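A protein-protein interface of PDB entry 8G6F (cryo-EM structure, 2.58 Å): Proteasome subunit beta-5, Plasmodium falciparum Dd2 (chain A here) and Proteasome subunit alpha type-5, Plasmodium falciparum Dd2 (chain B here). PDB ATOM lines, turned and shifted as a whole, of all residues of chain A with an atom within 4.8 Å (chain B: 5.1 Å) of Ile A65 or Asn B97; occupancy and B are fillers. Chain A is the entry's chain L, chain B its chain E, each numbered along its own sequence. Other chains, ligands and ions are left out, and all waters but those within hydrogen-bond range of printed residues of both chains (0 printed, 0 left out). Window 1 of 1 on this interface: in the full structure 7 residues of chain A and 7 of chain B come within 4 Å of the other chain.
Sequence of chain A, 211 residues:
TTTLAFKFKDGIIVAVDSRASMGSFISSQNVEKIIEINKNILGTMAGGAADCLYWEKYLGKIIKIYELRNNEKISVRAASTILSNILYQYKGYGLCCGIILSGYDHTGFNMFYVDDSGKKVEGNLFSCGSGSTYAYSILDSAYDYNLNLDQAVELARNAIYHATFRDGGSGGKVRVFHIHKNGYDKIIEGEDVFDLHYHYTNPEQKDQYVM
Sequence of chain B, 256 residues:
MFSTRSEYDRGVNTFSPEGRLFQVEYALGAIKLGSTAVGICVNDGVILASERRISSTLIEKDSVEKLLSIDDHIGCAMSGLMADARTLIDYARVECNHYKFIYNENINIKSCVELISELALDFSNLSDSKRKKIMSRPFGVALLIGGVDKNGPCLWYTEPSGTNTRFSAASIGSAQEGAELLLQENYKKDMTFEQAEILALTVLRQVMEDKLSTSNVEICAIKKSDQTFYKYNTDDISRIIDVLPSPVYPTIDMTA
O of Lys A61 sits at hydrogen-bond distance from ND2 of Asn B97.
CD of Lys A61 touches CB of Phe B101 (3.6 Å).
OD1 of Asn B97 touches CB of Lys A64, 3.4 Å away.
CD1 of Ile A65 touches O of Arg B93 (3.9 Å).
Ile A65 touches Val B94 (CD1 to N, 3.96 Å).
Asn B97 touches Ile A65.
CG of Leu A68 touches NE of Arg B93, 3.7 Å away.
Arg A69 touches Val B94 (NH1 to CG2, 3.6 Å).
Of chain B, only Arg B93 (3.9 Å), Val B94 (3.96 Å) and Asn B97 (3.4 Å) come within 4 Å of Ile A65.
Asn B97 touches three residues of chain A.
Of the printed residues of chain A, Arg B93 touches Ile A65 (3.9 Å) and Leu A68 (3.7 Å).
Of the printed residues of chain B, Lys A61 touches Asn B97 (2.8 Å) and Phe B101 (3.6 Å).
Of the printed residues of chain A, Val B94 touches Ile A65 (3.96 Å) and Arg A69 (3.6 Å).
Glu A67 touches none of the printed residues of chain B.
Ile A62 touches none of the printed residues of chain B.
The nearest printed residue of chain B that does not touch Ile A65 is Glu B95 (6.2 Å).
The nearest residue of chain A that does not touch Asn B97 is Ile A62 (4.7 Å).
Of the 10 printed residues of chain B, 4 touch a printed residue of chain A.
Hydrophobic or aromatic side chains of chain B that line the printed part of chain A: Val B94 and Phe B101.
Among the printed residues, no Asp or Glu carboxylate lies within 4 Å of a Lys or Arg side-chain nitrogen of the other chain.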
ATOM      1  N   LYS A  61      18.935  -2.016  -7.439  1.00  0.00           N
ATOM      2  CA  LYS A  61      18.574  -3.143  -6.581  1.00  0.00           C
ATOM      3  C   LYS A  61      17.114  -3.051  -6.148  1.00  0.00           C
ATOM      4  O   LYS A  61      16.368  -4.042  -6.192  1.00  0.00           O
ATOM      5  CB  LYS A  61      19.498  -3.186  -5.362  1.00  0.00           C
ATOM      6  CG  LYS A  61      19.020  -4.097  -4.238  1.00  0.00           C
ATOM      7  CD  LYS A  61      19.947  -4.077  -3.046  1.00  0.00           C
ATOM      8  CE  LYS A  61      19.801  -2.808  -2.237  1.00  0.00           C
ATOM      9  NZ  LYS A  61      19.017  -3.040  -0.998  1.00  0.00           N
ATOM     10  N   ILE A  62      16.688  -1.859  -5.724  1.00  0.00           N
ATOM     11  CA  ILE A  62      15.309  -1.686  -5.275  1.00  0.00           C
ATOM     12  C   ILE A  62      14.341  -1.957  -6.418  1.00  0.00           C
ATOM     13  O   ILE A  62      13.303  -2.604  -6.239  1.00  0.00           O
ATOM     14  CB  ILE A  62      15.110  -0.278  -4.689  1.00  0.00           C
ATOM     15  CG1 ILE A  62      15.854  -0.144  -3.365  1.00  0.00           C
ATOM     16  CG2 ILE A  62      13.638   0.009  -4.487  1.00  0.00           C
ATOM     17  CD1 ILE A  62      16.222   1.267  -3.031  1.00  0.00           C
ATOM     18  N   ILE A  63      14.661  -1.462  -7.610  1.00  0.00           N
ATOM     19  CA  ILE A  63      13.782  -1.653  -8.754  1.00  0.00           C
ATOM     20  C   ILE A  63      13.735  -3.118  -9.159  1.00  0.00           C
ATOM     21  O   ILE A  63      12.686  -3.628  -9.561  1.00  0.00           O
ATOM     22  CB  ILE A  63      14.233  -0.753  -9.914  1.00  0.00           C
ATOM     23  CG1 ILE A  63      13.892   0.699  -9.589  1.00  0.00           C
ATOM     24  CG2 ILE A  63      13.586  -1.202 -11.209  1.00  0.00           C
ATOM     25  CD1 ILE A  63      14.447   1.690 -10.558  1.00  0.00           C
ATOM     26  N   LYS A  64      14.865  -3.820  -9.071  1.00  0.00           N
ATOM     27  CA  LYS A  64      14.874  -5.237  -9.409  1.00  0.00           C
ATOM     28  C   LYS A  64      13.974  -6.022  -8.469  1.00  0.00           C
ATOM     29  O   LYS A  64      13.184  -6.866  -8.908  1.00  0.00           O
ATOM     30  CB  LYS A  64      16.300  -5.782  -9.361  1.00  0.00           C
ATOM     31  CG  LYS A  64      17.140  -5.436 -10.571  1.00  0.00           C
ATOM     32  CD  LYS A  64      18.602  -5.799 -10.351  1.00  0.00           C
ATOM     33  CE  LYS A  64      19.548  -4.876 -11.107  1.00  0.00           C
ATOM     34  NZ  LYS A  64      18.979  -4.366 -12.388  1.00  0.00           N
ATOM     35  N   ILE A  65      14.070  -5.756  -7.165  1.00  0.00           N
ATOM     36  CA  ILE A  65      13.229  -6.506  -6.236  1.00  0.00           C
ATOM     37  C   ILE A  65      11.762  -6.141  -6.431  1.00  0.00           C
ATOM     38  O   ILE A  65      10.882  -7.008  -6.372  1.00  0.00           O
ATOM     39  CB  ILE A  65      13.690  -6.302  -4.778  1.00  0.00           C
ATOM     40  CG1 ILE A  65      13.051  -7.348  -3.858  1.00  0.00           C
ATOM     41  CG2 ILE A  65      13.366  -4.916  -4.269  1.00  0.00           C
ATOM     42  CD1 ILE A  65      13.296  -8.782  -4.266  1.00  0.00           C
ATOM     43  N   TYR A  66      11.470  -4.863  -6.683  1.00  0.00           N
ATOM     44  CA  TYR A  66      10.090  -4.458  -6.926  1.00  0.00           C
ATOM     45  C   TYR A  66       9.520  -5.166  -8.149  1.00  0.00           C
ATOM     46  O   TYR A  66       8.393  -5.672  -8.123  1.00  0.00           O
ATOM     47  CB  TYR A  66      10.019  -2.940  -7.102  1.00  0.00           C
ATOM     48  CG  TYR A  66       8.723  -2.458  -7.710  1.00  0.00           C
ATOM     49  CD1 TYR A  66       7.634  -2.150  -6.910  1.00  0.00           C
ATOM     50  CD2 TYR A  66       8.587  -2.313  -9.080  1.00  0.00           C
ATOM     51  CE1 TYR A  66       6.453  -1.718  -7.458  1.00  0.00           C
ATOM     52  CE2 TYR A  66       7.408  -1.884  -9.635  1.00  0.00           C
ATOM     53  CZ  TYR A  66       6.345  -1.586  -8.820  1.00  0.00           C
ATOM     54  OH  TYR A  66       5.165  -1.152  -9.373  1.00  0.00           O
ATOM     55  N   GLU A  67      10.287  -5.198  -9.238  1.00  0.00           N
ATOM     56  CA  GLU A  67       9.820  -5.834 -10.463  1.00  0.00           C
ATOM     57  C   GLU A  67       9.632  -7.329 -10.270  1.00  0.00           C
ATOM     58  O   GLU A  67       8.663  -7.905 -10.771  1.00  0.00           O
ATOM     59  CB  GLU A  67      10.802  -5.560 -11.598  1.00  0.00           C
ATOM     60  CG  GLU A  67      10.364  -4.454 -12.531  1.00  0.00           C
ATOM     61  CD  GLU A  67      11.521  -3.671 -13.106  1.00  0.00           C
ATOM     62  OE1 GLU A  67      12.606  -4.257 -13.294  1.00  0.00           O
ATOM     63  OE2 GLU A  67      11.341  -2.468 -13.380  1.00  0.00           O
ATOM     64  N   LEU A  68      10.547  -7.977  -9.550  1.00  0.00           N
ATOM     65  CA  LEU A  68      10.394  -9.403  -9.296  1.00  0.00           C
ATOM     66  C   LEU A  68       9.143  -9.683  -8.477  1.00  0.00           C
ATOM     67  O   LEU A  68       8.401 -10.627  -8.768  1.00  0.00           O
ATOM     68  CB  LEU A  68      11.635  -9.940  -8.587  1.00  0.00           C
ATOM     69  CG  LEU A  68      11.778 -11.456  -8.457  1.00  0.00           C
ATOM     70  CD1 LEU A  68      11.506 -12.163  -9.769  1.00  0.00           C
ATOM     71  CD2 LEU A  68      13.162 -11.800  -7.955  1.00  0.00           C
ATOM     72  N   ARG A  69       8.885  -8.871  -7.451  1.00  0.00           N
ATOM     73  CA  ARG A  69       7.731  -9.118  -6.591  1.00  0.00           C
ATOM     74  C   ARG A  69       6.424  -8.872  -7.330  1.00  0.00           C
ATOM     75  O   ARG A  69       5.490  -9.674  -7.237  1.00  0.00           O
ATOM     76  CB  ARG A  69       7.806  -8.240  -5.345  1.00  0.00           C
ATOM     77  CG  ARG A  69       8.867  -8.666  -4.355  1.00  0.00           C
ATOM     78  CD  ARG A  69       8.602  -8.113  -2.969  1.00  0.00           C
ATOM     79  NE  ARG A  69       9.544  -7.061  -2.606  1.00  0.00           N
ATOM     80  CZ  ARG A  69      10.211  -6.996  -1.461  1.00  0.00           C
ATOM     81  NH1 ARG A  69      10.088  -7.926  -0.529  1.00  0.00           N
ATOM     82  NH2 ARG A  69      11.026  -5.969  -1.245  1.00  0.00           N
ATOM     83  N   ALA B  92      13.884 -15.419  -0.003  1.00  0.00           N
ATOM     84  CA  ALA B  92      14.925 -15.870  -0.921  1.00  0.00           C
ATOM     85  C   ALA B  92      15.149 -14.864  -2.042  1.00  0.00           C
ATOM     86  O   ALA B  92      16.291 -14.610  -2.437  1.00  0.00           O
ATOM     87  CB  ALA B  92      14.561 -17.237  -1.493  1.00  0.00           C
ATOM     88  N   ARG B  93      14.071 -14.292  -2.578  1.00  0.00           N
ATOM     89  CA  ARG B  93      14.204 -13.264  -3.602  1.00  0.00           C
ATOM     90  C   ARG B  93      14.995 -12.077  -3.076  1.00  0.00           C
ATOM     91  O   ARG B  93      15.901 -11.569  -3.746  1.00  0.00           O
ATOM     92  CB  ARG B  93      12.823 -12.806  -4.067  1.00  0.00           C
ATOM     93  CG  ARG B  93      12.087 -13.789  -4.938  1.00  0.00           C
ATOM     94  CD  ARG B  93      10.697 -13.282  -5.244  1.00  0.00           C
ATOM     95  NE  ARG B  93      10.095 -13.969  -6.378  1.00  0.00           N
ATOM     96  CZ  ARG B  93       8.810 -13.905  -6.691  1.00  0.00           C
ATOM     97  NH1 ARG B  93       7.957 -13.196  -5.973  1.00  0.00           N
ATOM     98  NH2 ARG B  93       8.370 -14.568  -7.755  1.00  0.00           N
ATOM     99  N   VAL B  94      14.662 -11.622  -1.870  1.00  0.00           N
ATOM    100  CA  VAL B  94      15.356 -10.473  -1.301  1.00  0.00           C
ATOM    101  C   VAL B  94      16.837 -10.776  -1.138  1.00  0.00           C
ATOM    102  O   VAL B  94      17.695  -9.943  -1.459  1.00  0.00           O
ATOM    103  CB  VAL B  94      14.709 -10.071   0.036  1.00  0.00           C
ATOM    104  CG1 VAL B  94      15.638  -9.174   0.829  1.00  0.00           C
ATOM    105  CG2 VAL B  94      13.388  -9.376  -0.211  1.00  0.00           C
ATOM    106  N   GLU B  95      17.167 -11.970  -0.645  1.00  0.00           N
ATOM    107  CA  GLU B  95      18.568 -12.282  -0.383  1.00  0.00           C
ATOM    108  C   GLU B  95      19.358 -12.471  -1.673  1.00  0.00           C
ATOM    109  O   GLU B  95      20.518 -12.055  -1.759  1.00  0.00           O
ATOM    110  CB  GLU B  95      18.674 -13.519   0.501  1.00  0.00           C
ATOM    111  CG  GLU B  95      18.348 -13.265   1.963  1.00  0.00           C
ATOM    112  CD  GLU B  95      19.049 -12.040   2.518  1.00  0.00           C
ATOM    113  OE1 GLU B  95      20.279 -11.926   2.341  1.00  0.00           O
ATOM    114  OE2 GLU B  95      18.369 -11.184   3.124  1.00  0.00           O
ATOM    115  N   CYS B  96      18.759 -13.095  -2.685  1.00  0.00           N
ATOM    116  CA  CYS B  96      19.441 -13.218  -3.969  1.00  0.00           C
ATOM    117  C   CYS B  96      19.662 -11.849  -4.599  1.00  0.00           C
ATOM    118  O   CYS B  96      20.721 -11.587  -5.185  1.00  0.00           O
ATOM    119  CB  CYS B  96      18.637 -14.120  -4.899  1.00  0.00           C
ATOM    120  SG  CYS B  96      18.584 -15.833  -4.362  1.00  0.00           S
ATOM    121  N   ASN B  97      18.677 -10.958  -4.480  1.00  0.00           N
ATOM    122  CA  ASN B  97      18.844  -9.597  -4.972  1.00  0.00           C
ATOM    123  C   ASN B  97      19.976  -8.884  -4.247  1.00  0.00           C
ATOM    124  O   ASN B  97      20.783  -8.185  -4.871  1.00  0.00           O
ATOM    125  CB  ASN B  97      17.532  -8.835  -4.802  1.00  0.00           C
ATOM    126  CG  ASN B  97      17.423  -7.652  -5.721  1.00  0.00           C
ATOM    127  OD1 ASN B  97      17.625  -7.767  -6.927  1.00  0.00           O
ATOM    128  ND2 ASN B  97      17.100  -6.500  -5.158  1.00  0.00           N
ATOM    129  N   HIS B  98      20.051  -9.041  -2.926  1.00  0.00           N
ATOM    130  CA  HIS B  98      21.114  -8.394  -2.165  1.00  0.00           C
ATOM    131  C   HIS B  98      22.483  -8.945  -2.545  1.00  0.00           C
ATOM    132  O   HIS B  98      23.459  -8.193  -2.634  1.00  0.00           O
ATOM    133  CB  HIS B  98      20.864  -8.570  -0.672  1.00  0.00           C
ATOM    134  CG  HIS B  98      21.883  -7.896   0.190  1.00  0.00           C
ATOM    135  ND1 HIS B  98      21.846  -6.549   0.470  1.00  0.00           N
ATOM    136  CD2 HIS B  98      22.970  -8.385   0.832  1.00  0.00           C
ATOM    137  CE1 HIS B  98      22.865  -6.236   1.248  1.00  0.00           C
ATOM    138  NE2 HIS B  98      23.562  -7.333   1.484  1.00  0.00           N
ATOM    139  N   TYR B  99      22.576 -10.258  -2.751  1.00  0.00           N
ATOM    140  CA  TYR B  99      23.830 -10.853  -3.197  1.00  0.00           C
ATOM    141  C   TYR B  99      24.249 -10.278  -4.540  1.00  0.00           C
ATOM    142  O   TYR B  99      25.423  -9.949  -4.753  1.00  0.00           O
ATOM    143  CB  TYR B  99      23.672 -12.371  -3.287  1.00  0.00           C
ATOM    144  CG  TYR B  99      24.890 -13.113  -3.795  1.00  0.00           C
ATOM    145  CD1 TYR B  99      25.243 -13.079  -5.136  1.00  0.00           C
ATOM    146  CD2 TYR B  99      25.672 -13.864  -2.935  1.00  0.00           C
ATOM    147  CE1 TYR B  99      26.343 -13.753  -5.596  1.00  0.00           C
ATOM    148  CE2 TYR B  99      26.771 -14.545  -3.391  1.00  0.00           C
ATOM    149  CZ  TYR B  99      27.102 -14.486  -4.720  1.00  0.00           C
ATOM    150  OH  TYR B  99      28.201 -15.168  -5.179  1.00  0.00           O
ATOM    151  N   LYS B 100      23.301 -10.171  -5.470  1.00  0.00           N
ATOM    152  CA  LYS B 100      23.614  -9.584  -6.765  1.00  0.00           C
ATOM    153  C   LYS B 100      24.084  -8.148  -6.603  1.00  0.00           C
ATOM    154  O   LYS B 100      24.999  -7.704  -7.301  1.00  0.00           O
ATOM    155  CB  LYS B 100      22.394  -9.652  -7.676  1.00  0.00           C
ATOM    156  CG  LYS B 100      22.731  -9.620  -9.148  1.00  0.00           C
ATOM    157  CD  LYS B 100      21.485  -9.641 -10.002  1.00  0.00           C
ATOM    158  CE  LYS B 100      20.726 -10.942  -9.848  1.00  0.00           C
ATOM    159  NZ  LYS B 100      19.700 -11.115 -10.907  1.00  0.00           N
ATOM    160  N   PHE B 101      23.474  -7.409  -5.681  1.00  0.00           N
ATOM    161  CA  PHE B 101      23.887  -6.031  -5.445  1.00  0.00           C
ATOM    162  C   PHE B 101      25.324  -5.962  -4.943  1.00  0.00           C
ATOM    163  O   PHE B 101      26.125  -5.161  -5.434  1.00  0.00           O
ATOM    164  CB  PHE B 101      22.943  -5.378  -4.444  1.00  0.00           C
ATOM    165  CG  PHE B 101      23.391  -4.025  -3.982  1.00  0.00           C
ATOM    166  CD1 PHE B 101      23.365  -2.945  -4.840  1.00  0.00           C
ATOM    167  CD2 PHE B 101      23.819  -3.829  -2.684  1.00  0.00           C
ATOM    168  CE1 PHE B 101      23.768  -1.703  -4.418  1.00  0.00           C
ATOM    169  CE2 PHE B 101      24.225  -2.585  -2.258  1.00  0.00           C
ATOM    170  CZ  PHE B 101      24.198  -1.522  -3.128  1.00  0.00           C
